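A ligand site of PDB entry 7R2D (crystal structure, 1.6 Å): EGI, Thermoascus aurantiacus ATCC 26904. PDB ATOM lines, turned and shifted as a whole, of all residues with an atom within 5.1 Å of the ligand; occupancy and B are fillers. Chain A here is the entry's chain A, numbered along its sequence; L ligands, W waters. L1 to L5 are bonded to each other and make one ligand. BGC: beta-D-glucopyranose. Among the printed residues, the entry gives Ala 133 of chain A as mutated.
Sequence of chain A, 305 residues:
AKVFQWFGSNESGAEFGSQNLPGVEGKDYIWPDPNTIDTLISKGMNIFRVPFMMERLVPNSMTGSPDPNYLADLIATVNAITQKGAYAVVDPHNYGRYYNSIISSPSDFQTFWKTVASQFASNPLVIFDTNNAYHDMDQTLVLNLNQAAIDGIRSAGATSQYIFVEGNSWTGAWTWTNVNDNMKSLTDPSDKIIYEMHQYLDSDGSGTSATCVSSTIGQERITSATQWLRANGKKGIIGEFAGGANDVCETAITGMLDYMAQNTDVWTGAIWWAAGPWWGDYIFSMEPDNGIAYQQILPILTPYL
The backbone carbonyl oxygen (O) of Lys 27 sits at hydrogen-bond distance from an oxygen (O2) of BGC L5 (2.5 Å).
The side-chain carboxylate (OE2) of Glu 240 is in hydrogen-bond range of an oxygen (O2) of BGC L1 (3.0 Å).
An oxygen (O4) of BGC L1 sits at hydrogen-bond distance from the indole nitrogen (NE1) of Trp 273.
O6 of BGC L4 lies within hydrogen-bond range of O of Asp 28 (2.6 Å).
An oxygen (O6) of BGC L2 lies within hydrogen-bond range of the side-chain carboxylate of Glu 15.
O2 of BGC L1 sits at hydrogen-bond distance from NE2 of His 93, at 3.0 Å.
The backbone carbonyl oxygen (O) of Ser 206 is in hydrogen-bond range of an oxygen (O6) of BGC L1, at 2.9 Å.
O2 of BGC L1 sits at hydrogen-bond distance from ND2 of Asn 132 (2.9 Å).
OH of Tyr 95 sits at hydrogen-bond distance from O3 of BGC L1.
An oxygen (O2) of BGC L3 sits at hydrogen-bond distance from the backbone NH (N) of Gly 17.
An oxygen (O6) of BGC L5 lies within hydrogen-bond range of the indole nitrogen (NE1) of Trp 278, at 3.2 Å.
OH of Tyr 282 sits at hydrogen-bond distance from NE1 of Trp 273, at 3.0 Å.
The side-chain hydroxyl (OH) of Tyr 200 sits at hydrogen-bond distance from the side-chain carboxylate (OE1) of Glu 240, at 2.6 Å.
OE2 of Glu 240 lies close to OD1 of Asn 132 (3.3 Å).
The side-chain hydroxyl (OG) of Ser 12 is in hydrogen-bond range of the side-chain carboxylate (OE2) of Glu 15.
The side-chain hydroxyl of Ser 206 sits at hydrogen-bond distance from the side-chain hydroxyl of Thr 208 (2.8 Å).
O of Asn 132 is in hydrogen-bond range of N of Tyr 95.
NE2 of His 93 sits close to ND2 of Asn 132 (3.2 Å).
Merely in contact with the ligand: Phe 16, Gly 26, Tyr 200, Gly 207, Thr 208, Trp 279 and Tyr 282.
Hydrophobic or aromatic side chains that line the ligand: Phe 16, His 93, Tyr 200, Trp 273, Trp 278 and Trp 279.
18 residues have an atom within 4 Å of the ligand: Glu 15, Phe 16, Gly 17, Gly 26, Lys 27, Asp 28, His 93, Tyr 95, Asn 132, Tyr 200, Ser 206, Gly 207, Thr 208, Glu 240, Trp 273, Trp 278, Trp 279 and Tyr 282.
Water W4 bridges O3 of BGC L5 and O of Gly 26.
Water W13 lies within hydrogen-bond range of O of Trp 278 (2.6 Å), O2 of BGC L4 (2.7 Å) and O of Trp 279 (3.2 Å).
Water W6 lies within hydrogen-bond range of O of Ser 206 (2.6 Å) and O5 of BGC L1 (2.7 Å).
Water W3 lies within hydrogen-bond range of OH of Tyr 282 (2.7 Å), O of Gly 207 (2.7 Å) and O2 of BGC L2 (2.8 Å).
Water W5 bridges an oxygen (O3) of BGC L4 (2.8 Å) and the backbone carbonyl oxygen of Trp 278 (3.1 Å).
Water W15 lies within hydrogen-bond range of N of Ser 18 (2.8 Å), O2 of BGC L3 (3.3 Å) and N of Gly 17 (3.4 Å).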
ATOM      1  N   SER A  12      22.646 -27.400 -19.307  1.00  0.00           N
ATOM      2  CA  SER A  12      23.432 -27.210 -20.520  1.00  0.00           C
ATOM      3  C   SER A  12      22.543 -26.845 -21.708  1.00  0.00           C
ATOM      4  O   SER A  12      21.371 -27.251 -21.780  1.00  0.00           O
ATOM      5  CB  SER A  12      24.213 -28.482 -20.835  1.00  0.00           C
ATOM      6  OG  SER A  12      24.994 -28.358 -22.016  1.00  0.00           O
ATOM      7  N   GLU A  15      25.680 -23.229 -24.571  1.00  0.00           N
ATOM      8  CA  GLU A  15      26.996 -23.397 -25.159  1.00  0.00           C
ATOM      9  C   GLU A  15      26.982 -24.401 -26.301  1.00  0.00           C
ATOM     10  O   GLU A  15      28.042 -24.707 -26.857  1.00  0.00           O
ATOM     11  CB  GLU A  15      27.993 -23.836 -24.059  1.00  0.00           C
ATOM     12  CG  GLU A  15      28.078 -25.351 -23.786  1.00  0.00           C
ATOM     13  CD  GLU A  15      26.903 -25.934 -22.990  1.00  0.00           C
ATOM     14  OE1 GLU A  15      25.798 -25.353 -22.974  1.00  0.00           O
ATOM     15  OE2 GLU A  15      27.069 -27.043 -22.446  1.00  0.00           O
ATOM     16  N   PHE A  16      25.819 -24.908 -26.675  1.00  0.00           N
ATOM     17  CA  PHE A  16      25.695 -25.918 -27.707  1.00  0.00           C
ATOM     18  C   PHE A  16      26.082 -25.338 -29.061  1.00  0.00           C
ATOM     19  O   PHE A  16      26.009 -24.122 -29.293  1.00  0.00           O
ATOM     20  CB  PHE A  16      24.249 -26.427 -27.792  1.00  0.00           C
ATOM     21  CG  PHE A  16      23.965 -27.611 -26.901  1.00  0.00           C
ATOM     22  CD1 PHE A  16      24.694 -27.829 -25.745  1.00  0.00           C
ATOM     23  CD2 PHE A  16      22.959 -28.501 -27.243  1.00  0.00           C
ATOM     24  CE1 PHE A  16      24.407 -28.921 -24.937  1.00  0.00           C
ATOM     25  CE2 PHE A  16      22.672 -29.593 -26.435  1.00  0.00           C
ATOM     26  CZ  PHE A  16      23.396 -29.802 -25.282  1.00  0.00           C
ATOM     27  N   GLY A  17      26.471 -26.208 -29.983  1.00  0.00           N
ATOM     28  CA  GLY A  17      26.737 -25.774 -31.358  1.00  0.00           C
ATOM     29  C   GLY A  17      27.814 -24.712 -31.457  1.00  0.00           C
ATOM     30  O   GLY A  17      27.661 -23.766 -32.244  1.00  0.00           O
ATOM     31  N   SER A  18      28.889 -24.859 -30.682  1.00  0.00           N
ATOM     32  CA  SER A  18      29.939 -23.853 -30.545  1.00  0.00           C
ATOM     33  C   SER A  18      30.698 -23.610 -31.841  1.00  0.00           C
ATOM     34  O   SER A  18      31.438 -22.622 -31.931  1.00  0.00           O
ATOM     35  CB  SER A  18      30.907 -24.259 -29.439  1.00  0.00           C
ATOM     36  OG  SER A  18      31.599 -25.461 -29.746  1.00  0.00           O
ATOM     37  N   GLY A  26      17.806 -21.002 -30.699  1.00  0.00           N
ATOM     38  CA  GLY A  26      16.745 -21.843 -31.221  1.00  0.00           C
ATOM     39  C   GLY A  26      17.164 -22.714 -32.377  1.00  0.00           C
ATOM     40  O   GLY A  26      16.380 -23.572 -32.814  1.00  0.00           O
ATOM     41  N   LYS A  27      18.377 -22.529 -32.898  1.00  0.00           N
ATOM     42  CA  LYS A  27      18.935 -23.402 -33.920  1.00  0.00           C
ATOM     43  C   LYS A  27      20.263 -23.999 -33.471  1.00  0.00           C
ATOM     44  O   LYS A  27      20.394 -25.224 -33.436  1.00  0.00           O
ATOM     45  CB  LYS A  27      19.086 -22.612 -35.235  1.00  0.00           C
ATOM     46  CG  LYS A  27      19.735 -23.352 -36.391  1.00  0.00           C
ATOM     47  CD  LYS A  27      20.080 -22.382 -37.509  1.00  0.00           C
ATOM     48  CE  LYS A  27      20.574 -23.101 -38.750  1.00  0.00           C
ATOM     49  NZ  LYS A  27      20.303 -24.557 -38.684  1.00  0.00           N
ATOM     50  N   ASP A  28      21.232 -23.164 -33.080  1.00  0.00           N
ATOM     51  CA  ASP A  28      22.539 -23.658 -32.620  1.00  0.00           C
ATOM     52  C   ASP A  28      22.565 -23.942 -31.131  1.00  0.00           C
ATOM     53  O   ASP A  28      23.248 -24.883 -30.681  1.00  0.00           O
ATOM     54  CB  ASP A  28      23.611 -22.627 -32.973  1.00  0.00           C
ATOM     55  CG  ASP A  28      23.775 -22.449 -34.471  1.00  0.00           C
ATOM     56  OD1 ASP A  28      24.056 -23.442 -35.165  1.00  0.00           O
ATOM     57  OD2 ASP A  28      23.530 -21.318 -34.955  1.00  0.00           O
ATOM     58  N   TYR A  29      21.846 -23.152 -30.334  1.00  0.00           N
ATOM     59  CA  TYR A  29      21.860 -23.273 -28.887  1.00  0.00           C
ATOM     60  C   TYR A  29      20.490 -22.908 -28.342  1.00  0.00           C
ATOM     61  O   TYR A  29      19.658 -22.335 -29.044  1.00  0.00           O
ATOM     62  CB  TYR A  29      22.940 -22.378 -28.276  1.00  0.00           C
ATOM     63  CG  TYR A  29      22.766 -20.899 -28.564  1.00  0.00           C
ATOM     64  CD1 TYR A  29      21.974 -20.099 -27.750  1.00  0.00           C
ATOM     65  CD2 TYR A  29      23.392 -20.301 -29.662  1.00  0.00           C
ATOM     66  CE1 TYR A  29      21.804 -18.745 -28.012  1.00  0.00           C
ATOM     67  CE2 TYR A  29      23.229 -18.940 -29.921  1.00  0.00           C
ATOM     68  CZ  TYR A  29      22.440 -18.171 -29.093  1.00  0.00           C
ATOM     69  OH  TYR A  29      22.273 -16.818 -29.331  1.00  0.00           O
ATOM     70  N   HIS A  93      31.729 -21.429 -20.342  1.00  0.00           N
ATOM     71  CA  HIS A  93      32.137 -22.792 -20.634  1.00  0.00           C
ATOM     72  C   HIS A  93      33.216 -22.840 -21.717  1.00  0.00           C
ATOM     73  O   HIS A  93      33.035 -23.417 -22.783  1.00  0.00           O
ATOM     74  CB  HIS A  93      30.914 -23.594 -21.073  1.00  0.00           C
ATOM     75  CG  HIS A  93      30.949 -25.032 -20.667  1.00  0.00           C
ATOM     76  ND1 HIS A  93      30.836 -25.455 -19.357  1.00  0.00           N
ATOM     77  CD2 HIS A  93      31.067 -26.148 -21.417  1.00  0.00           C
ATOM     78  CE1 HIS A  93      30.888 -26.782 -19.331  1.00  0.00           C
ATOM     79  NE2 HIS A  93      31.034 -27.223 -20.560  1.00  0.00           N
ATOM     80  N   TYR A  95      36.994 -23.356 -21.427  1.00  0.00           N
ATOM     81  CA  TYR A  95      38.230 -24.140 -21.484  1.00  0.00           C
ATOM     82  C   TYR A  95      39.458 -23.248 -21.499  1.00  0.00           C
ATOM     83  O   TYR A  95      40.500 -23.610 -22.041  1.00  0.00           O
ATOM     84  CB  TYR A  95      38.219 -25.059 -22.705  1.00  0.00           C
ATOM     85  CG  TYR A  95      36.978 -25.944 -22.754  1.00  0.00           C
ATOM     86  CD1 TYR A  95      36.919 -27.102 -21.980  1.00  0.00           C
ATOM     87  CD2 TYR A  95      35.881 -25.606 -23.543  1.00  0.00           C
ATOM     88  CE1 TYR A  95      35.815 -27.915 -22.000  1.00  0.00           C
ATOM     89  CE2 TYR A  95      34.747 -26.415 -23.568  1.00  0.00           C
ATOM     90  CZ  TYR A  95      34.734 -27.580 -22.791  1.00  0.00           C
ATOM     91  OH  TYR A  95      33.625 -28.393 -22.802  1.00  0.00           O
ATOM     92  N   ASN A 132      35.273 -22.899 -17.412  1.00  0.00           N
ATOM     93  CA  ASN A 132      35.129 -24.342 -17.367  1.00  0.00           C
ATOM     94  C   ASN A 132      36.405 -25.021 -17.860  1.00  0.00           C
ATOM     95  O   ASN A 132      36.837 -24.779 -18.993  1.00  0.00           O
ATOM     96  CB  ASN A 132      33.936 -24.789 -18.215  1.00  0.00           C
ATOM     97  CG  ASN A 132      33.833 -26.301 -18.296  1.00  0.00           C
ATOM     98  OD1 ASN A 132      33.559 -26.936 -17.301  1.00  0.00           O
ATOM     99  ND2 ASN A 132      34.032 -26.875 -19.472  1.00  0.00           N
ATOM    100  N   ALA A 133      36.994 -25.869 -17.016  1.00  0.00           N
ATOM    101  CA  ALA A 133      37.923 -26.911 -17.434  1.00  0.00           C
ATOM    102  C   ALA A 133      39.091 -26.388 -18.279  1.00  0.00           C
ATOM    103  O   ALA A 133      39.315 -26.818 -19.408  1.00  0.00           O
ATOM    104  CB  ALA A 133      37.157 -28.006 -18.190  1.00  0.00           C
ATOM    105  N   TRP A 170      41.672 -30.125 -17.222  1.00  0.00           N
ATOM    106  CA  TRP A 170      40.217 -30.181 -17.303  1.00  0.00           C
ATOM    107  C   TRP A 170      39.583 -30.140 -15.917  1.00  0.00           C
ATOM    108  O   TRP A 170      38.498 -30.673 -15.700  1.00  0.00           O
ATOM    109  CB  TRP A 170      39.729 -31.407 -18.088  1.00  0.00           C
ATOM    110  CG  TRP A 170      40.439 -31.644 -19.396  1.00  0.00           C
ATOM    111  CD1 TRP A 170      41.637 -32.290 -19.589  1.00  0.00           C
ATOM    112  CD2 TRP A 170      40.011 -31.209 -20.685  1.00  0.00           C
ATOM    113  NE1 TRP A 170      41.953 -32.303 -20.922  1.00  0.00           N
ATOM    114  CE2 TRP A 170      40.986 -31.640 -21.618  1.00  0.00           C
ATOM    115  CE3 TRP A 170      38.899 -30.493 -21.142  1.00  0.00           C
ATOM    116  CZ2 TRP A 170      40.864 -31.387 -22.988  1.00  0.00           C
ATOM    117  CZ3 TRP A 170      38.789 -30.241 -22.505  1.00  0.00           C
ATOM    118  CH2 TRP A 170      39.760 -30.688 -23.406  1.00  0.00           C
ATOM    119  N   HIS A 198      36.111 -31.584 -11.437  1.00  0.00           N
ATOM    120  CA  HIS A 198      35.212 -32.477 -12.154  1.00  0.00           C
ATOM    121  C   HIS A 198      35.712 -33.911 -12.041  1.00  0.00           C
ATOM    122  O   HIS A 198      36.915 -34.151 -12.005  1.00  0.00           O
ATOM    123  CB  HIS A 198      35.136 -32.136 -13.637  1.00  0.00           C
ATOM    124  CG  HIS A 198      34.635 -30.739 -13.922  1.00  0.00           C
ATOM    125  ND1 HIS A 198      34.684 -30.189 -15.177  1.00  0.00           N
ATOM    126  CD2 HIS A 198      34.107 -29.798 -13.111  1.00  0.00           C
ATOM    127  CE1 HIS A 198      34.186 -28.960 -15.139  1.00  0.00           C
ATOM    128  NE2 HIS A 198      33.829 -28.698 -13.899  1.00  0.00           N
ATOM    129  N   TYR A 200      34.784 -37.773 -13.815  1.00  0.00           N
ATOM    130  CA  TYR A 200      34.044 -38.773 -14.558  1.00  0.00           C
ATOM    131  C   TYR A 200      34.639 -40.133 -14.268  1.00  0.00           C
ATOM    132  O   TYR A 200      35.698 -40.252 -13.661  1.00  0.00           O
ATOM    133  CB  TYR A 200      34.072 -38.432 -16.052  1.00  0.00           C
ATOM    134  CG  TYR A 200      33.231 -37.209 -16.329  1.00  0.00           C
ATOM    135  CD1 TYR A 200      31.843 -37.281 -16.327  1.00  0.00           C
ATOM    136  CD2 TYR A 200      33.822 -35.977 -16.514  1.00  0.00           C
ATOM    137  CE1 TYR A 200      31.059 -36.155 -16.561  1.00  0.00           C
ATOM    138  CE2 TYR A 200      33.042 -34.824 -16.745  1.00  0.00           C
ATOM    139  CZ  TYR A 200      31.662 -34.938 -16.773  1.00  0.00           C
ATOM    140  OH  TYR A 200      30.881 -33.826 -17.017  1.00  0.00           O
ATOM    141  N   SER A 206      37.068 -39.022 -19.399  1.00  0.00           N
ATOM    142  CA  SER A 206      36.536 -37.987 -20.269  1.00  0.00           C
ATOM    143  C   SER A 206      35.032 -37.803 -20.105  1.00  0.00           C
ATOM    144  O   SER A 206      34.481 -36.807 -20.597  1.00  0.00           O
ATOM    145  CB  SER A 206      36.841 -38.311 -21.731  1.00  0.00           C
ATOM    146  OG  SER A 206      36.159 -39.487 -22.133  1.00  0.00           O
ATOM    147  N   GLY A 207      34.352 -38.735 -19.434  1.00  0.00           N
ATOM    148  CA  GLY A 207      32.904 -38.696 -19.363  1.00  0.00           C
ATOM    149  C   GLY A 207      32.224 -38.764 -20.719  1.00  0.00           C
ATOM    150  O   GLY A 207      31.281 -38.016 -20.969  1.00  0.00           O
ATOM    151  N   THR A 208      32.700 -39.628 -21.604  1.00  0.00           N
ATOM    152  CA  THR A 208      32.067 -39.794 -22.899  1.00  0.00           C
ATOM    153  C   THR A 208      31.491 -41.186 -23.092  1.00  0.00           C
ATOM    154  O   THR A 208      30.854 -41.443 -24.114  1.00  0.00           O
ATOM    155  CB  THR A 208      33.031 -39.478 -24.037  1.00  0.00           C
ATOM    156  OG1 THR A 208      34.203 -40.298 -23.945  1.00  0.00           O
ATOM    157  CG2 THR A 208      33.431 -37.991 -23.998  1.00  0.00           C
ATOM    158  N   GLU A 240      31.077 -31.116 -11.927  1.00  0.00           N
ATOM    159  CA  GLU A 240      30.509 -32.038 -12.896  1.00  0.00           C
ATOM    160  C   GLU A 240      30.865 -33.444 -12.485  1.00  0.00           C
ATOM    161  O   GLU A 240      32.030 -33.727 -12.185  1.00  0.00           O
ATOM    162  CB  GLU A 240      31.018 -31.828 -14.329  1.00  0.00           C
ATOM    163  CG  GLU A 240      30.880 -30.441 -14.905  1.00  0.00           C
ATOM    164  CD  GLU A 240      31.351 -30.382 -16.347  1.00  0.00           C
ATOM    165  OE1 GLU A 240      31.800 -31.419 -16.870  1.00  0.00           O
ATOM    166  OE2 GLU A 240      31.353 -29.302 -16.924  1.00  0.00           O
ATOM    167  N   TRP A 273      26.336 -33.722 -14.347  1.00  0.00           N
ATOM    168  CA  TRP A 273      26.380 -33.340 -15.753  1.00  0.00           C
ATOM    169  C   TRP A 273      25.563 -34.362 -16.526  1.00  0.00           C
ATOM    170  O   TRP A 273      25.963 -35.523 -16.618  1.00  0.00           O
ATOM    171  CB  TRP A 273      27.823 -33.301 -16.294  1.00  0.00           C
ATOM    172  CG  TRP A 273      27.830 -32.932 -17.742  1.00  0.00           C
ATOM    173  CD1 TRP A 273      27.701 -33.766 -18.824  1.00  0.00           C
ATOM    174  CD2 TRP A 273      27.912 -31.601 -18.277  1.00  0.00           C
ATOM    175  NE1 TRP A 273      27.713 -33.037 -19.997  1.00  0.00           N
ATOM    176  CE2 TRP A 273      27.837 -31.703 -19.687  1.00  0.00           C
ATOM    177  CE3 TRP A 273      28.040 -30.343 -17.701  1.00  0.00           C
ATOM    178  CZ2 TRP A 273      27.883 -30.588 -20.525  1.00  0.00           C
ATOM    179  CZ3 TRP A 273      28.103 -29.231 -18.541  1.00  0.00           C
ATOM    180  CH2 TRP A 273      28.012 -29.375 -19.937  1.00  0.00           C
ATOM    181  N   TRP A 278      18.026 -29.905 -24.835  1.00  0.00           N
ATOM    182  CA  TRP A 278      18.348 -30.451 -26.149  1.00  0.00           C
ATOM    183  C   TRP A 278      19.237 -31.694 -26.086  1.00  0.00           C
ATOM    184  O   TRP A 278      19.970 -31.996 -27.027  1.00  0.00           O
ATOM    185  CB  TRP A 278      19.012 -29.400 -27.046  1.00  0.00           C
ATOM    186  CG  TRP A 278      18.032 -28.445 -27.695  1.00  0.00           C
ATOM    187  CD1 TRP A 278      16.671 -28.418 -27.531  1.00  0.00           C
ATOM    188  CD2 TRP A 278      18.345 -27.405 -28.625  1.00  0.00           C
ATOM    189  NE1 TRP A 278      16.126 -27.411 -28.282  1.00  0.00           N
ATOM    190  CE2 TRP A 278      17.128 -26.775 -28.968  1.00  0.00           C
ATOM    191  CE3 TRP A 278      19.532 -26.941 -29.185  1.00  0.00           C
ATOM    192  CZ2 TRP A 278      17.066 -25.712 -29.865  1.00  0.00           C
ATOM    193  CZ3 TRP A 278      19.470 -25.879 -30.082  1.00  0.00           C
ATOM    194  CH2 TRP A 278      18.247 -25.270 -30.405  1.00  0.00           C
ATOM    195  N   TRP A 279      19.191 -32.441 -24.976  1.00  0.00           N
ATOM    196  CA  TRP A 279      20.046 -33.606 -24.840  1.00  0.00           C
ATOM    197  C   TRP A 279      19.455 -34.849 -25.488  1.00  0.00           C
ATOM    198  O   TRP A 279      20.200 -35.794 -25.791  1.00  0.00           O
ATOM    199  CB  TRP A 279      20.279 -33.884 -23.352  1.00  0.00           C
ATOM    200  CG  TRP A 279      21.335 -33.024 -22.696  1.00  0.00           C
ATOM    201  CD1 TRP A 279      21.151 -32.224 -21.605  1.00  0.00           C
ATOM    202  CD2 TRP A 279      22.723 -32.913 -23.041  1.00  0.00           C
ATOM    203  NE1 TRP A 279      22.337 -31.612 -21.253  1.00  0.00           N
ATOM    204  CE2 TRP A 279      23.312 -32.019 -22.118  1.00  0.00           C
ATOM    205  CE3 TRP A 279      23.525 -33.486 -24.034  1.00  0.00           C
ATOM    206  CZ2 TRP A 279      24.673 -31.682 -22.159  1.00  0.00           C
ATOM    207  CZ3 TRP A 279      24.869 -33.147 -24.073  1.00  0.00           C
ATOM    208  CH2 TRP A 279      25.428 -32.257 -23.143  1.00  0.00           C
ATOM    209  N   TYR A 282      20.743 -38.491 -24.652  1.00  0.00           N
ATOM    210  CA  TYR A 282      22.052 -38.439 -24.012  1.00  0.00           C
ATOM    211  C   TYR A 282      22.153 -39.386 -22.821  1.00  0.00           C
ATOM    212  O   TYR A 282      21.262 -39.426 -21.975  1.00  0.00           O
ATOM    213  CB  TYR A 282      22.295 -36.995 -23.569  1.00  0.00           C
ATOM    214  CG  TYR A 282      23.670 -36.667 -23.031  1.00  0.00           C
ATOM    215  CD1 TYR A 282      24.822 -37.072 -23.684  1.00  0.00           C
ATOM    216  CD2 TYR A 282      23.787 -35.877 -21.911  1.00  0.00           C
ATOM    217  CE1 TYR A 282      26.066 -36.721 -23.196  1.00  0.00           C
ATOM    218  CE2 TYR A 282      25.027 -35.504 -21.425  1.00  0.00           C
ATOM    219  CZ  TYR A 282      26.159 -35.943 -22.066  1.00  0.00           C
ATOM    220  OH  TYR A 282      27.389 -35.570 -21.563  1.00  0.00           O
HETATM  221  C2  BGC L   1      32.831 -30.658 -20.325  1.00  0.00           C
HETATM  222  C3  BGC L   1      31.468 -31.004 -20.935  1.00  0.00           C
HETATM  223  C4  BGC L   1      31.510 -32.397 -21.565  1.00  0.00           C
HETATM  224  C5  BGC L   1      31.914 -33.358 -20.469  1.00  0.00           C
HETATM  225  C6  BGC L   1      31.895 -34.807 -20.904  1.00  0.00           C
HETATM  226  C1  BGC L   1      33.377 -31.775 -19.435  1.00  0.00           C
HETATM  227  O1  BGC L   1      34.722 -31.499 -19.199  1.00  0.00           O
HETATM  228  O2  BGC L   1      32.745 -29.455 -19.558  1.00  0.00           O
HETATM  229  O3  BGC L   1      31.107 -29.996 -21.871  1.00  0.00           O
HETATM  230  O4  BGC L   1      30.261 -32.821 -22.113  1.00  0.00           O
HETATM  231  O5  BGC L   1      33.258 -33.051 -20.074  1.00  0.00           O
HETATM  232  O6  BGC L   1      32.735 -34.974 -22.038  1.00  0.00           O
HETATM  233  C2  BGC L   2      29.368 -33.515 -24.300  1.00  0.00           C
HETATM  234  C3  BGC L   2      28.986 -33.000 -25.689  1.00  0.00           C
HETATM  235  C4  BGC L   2      28.285 -31.643 -25.627  1.00  0.00           C
HETATM  236  C5  BGC L   2      29.051 -30.681 -24.721  1.00  0.00           C
HETATM  237  C6  BGC L   2      28.317 -29.374 -24.495  1.00  0.00           C
HETATM  238  C1  BGC L   2      30.059 -32.429 -23.470  1.00  0.00           C
HETATM  239  O2  BGC L   2      30.238 -34.641 -24.430  1.00  0.00           O
HETATM  240  O3  BGC L   2      28.143 -33.942 -26.330  1.00  0.00           O
HETATM  241  O4  BGC L   2      28.268 -31.066 -26.930  1.00  0.00           O
HETATM  242  O5  BGC L   2      29.227 -31.279 -23.445  1.00  0.00           O
HETATM  243  O6  BGC L   2      29.024 -28.562 -23.563  1.00  0.00           O
HETATM  244  C2  BGC L   3      26.859 -30.081 -28.614  1.00  0.00           C
HETATM  245  C3  BGC L   3      25.432 -29.997 -29.114  1.00  0.00           C
HETATM  246  C4  BGC L   3      24.837 -31.393 -29.318  1.00  0.00           C
HETATM  247  C5  BGC L   3      25.090 -32.284 -28.100  1.00  0.00           C
HETATM  248  C6  BGC L   3      24.724 -33.733 -28.337  1.00  0.00           C
HETATM  249  C1  BGC L   3      26.914 -30.967 -27.379  1.00  0.00           C
HETATM  250  O2  BGC L   3      27.336 -28.783 -28.303  1.00  0.00           O
HETATM  251  O3  BGC L   3      25.407 -29.226 -30.309  1.00  0.00           O
HETATM  252  O4  BGC L   3      23.416 -31.340 -29.393  1.00  0.00           O
HETATM  253  O5  BGC L   3      26.464 -32.260 -27.721  1.00  0.00           O
HETATM  254  O6  BGC L   3      25.498 -34.276 -29.403  1.00  0.00           O
HETATM  255  C2  BGC L   4      21.521 -31.670 -30.753  1.00  0.00           C
HETATM  256  C3  BGC L   4      20.787 -31.229 -32.004  1.00  0.00           C
HETATM  257  C4  BGC L   4      20.737 -29.712 -32.088  1.00  0.00           C
HETATM  258  C5  BGC L   4      22.154 -29.157 -31.996  1.00  0.00           C
HETATM  259  C6  BGC L   4      22.224 -27.656 -31.991  1.00  0.00           C
HETATM  260  C1  BGC L   4      22.884 -30.999 -30.658  1.00  0.00           C
HETATM  261  O2  BGC L   4      21.703 -33.077 -30.769  1.00  0.00           O
HETATM  262  O3  BGC L   4      19.474 -31.777 -32.016  1.00  0.00           O
HETATM  263  O4  BGC L   4      20.143 -29.328 -33.330  1.00  0.00           O
HETATM  264  O5  BGC L   4      22.752 -29.590 -30.763  1.00  0.00           O
HETATM  265  O6  BGC L   4      23.572 -27.215 -31.857  1.00  0.00           O
HETATM  266  C2  BGC L   5      18.535 -27.942 -34.430  1.00  0.00           C
HETATM  267  C3  BGC L   5      17.252 -27.152 -34.273  1.00  0.00           C
HETATM  268  C4  BGC L   5      16.172 -28.016 -33.641  1.00  0.00           C
HETATM  269  C5  BGC L   5      16.681 -28.643 -32.341  1.00  0.00           C
HETATM  270  C6  BGC L   5      15.714 -29.667 -31.804  1.00  0.00           C
HETATM  271  C1  BGC L   5      18.963 -28.545 -33.094  1.00  0.00           C
HETATM  272  O2  BGC L   5      19.563 -27.101 -34.931  1.00  0.00           O
HETATM  273  O3  BGC L   5      16.822 -26.703 -35.552  1.00  0.00           O
HETATM  274  O4  BGC L   5      15.021 -27.233 -33.354  1.00  0.00           O
HETATM  275  O5  BGC L   5      17.914 -29.341 -32.570  1.00  0.00           O
HETATM  276  O6  BGC L   5      15.867 -29.841 -30.406  1.00  0.00           O
HETATM  277  O   HOH W   1      36.255 -31.470 -17.031  1.00  0.00           O
HETATM  278  O   HOH W   2      35.845 -31.946 -21.979  1.00  0.00           O
HETATM  279  O   HOH W   3      29.596 -36.636 -22.613  1.00  0.00           O
HETATM  280  O   HOH W   4      15.323 -24.517 -35.455  1.00  0.00           O
HETATM  281  O   HOH W   5      18.141 -31.759 -29.519  1.00  0.00           O
HETATM  282  O   HOH W   6      35.464 -34.582 -19.752  1.00  0.00           O
HETATM  283  O   HOH W   7      24.059 -34.203 -32.079  1.00  0.00           O
HETATM  284  O   HOH W   8      21.807 -28.502 -35.776  1.00  0.00           O
HETATM  285  O   HOH W   9      24.861 -27.256 -33.955  1.00  0.00           O
HETATM  286  O   HOH W  10      29.985 -28.398 -27.921  1.00  0.00           O
HETATM  287  O   HOH W  11      32.811 -34.184 -25.665  1.00  0.00           O
HETATM  288  O   HOH W  12      19.445 -34.682 -32.194  1.00  0.00           O
HETATM  289  O   HOH W  13      20.727 -34.064 -28.468  1.00  0.00           O
HETATM  290  O   HOH W  14      27.252 -29.576 -32.110  1.00  0.00           O
HETATM  291  O   HOH W  15      29.467 -27.627 -30.505  1.00  0.00           O
HETATM  292  O   HOH W  16      31.452 -27.572 -24.460  1.00  0.00           O
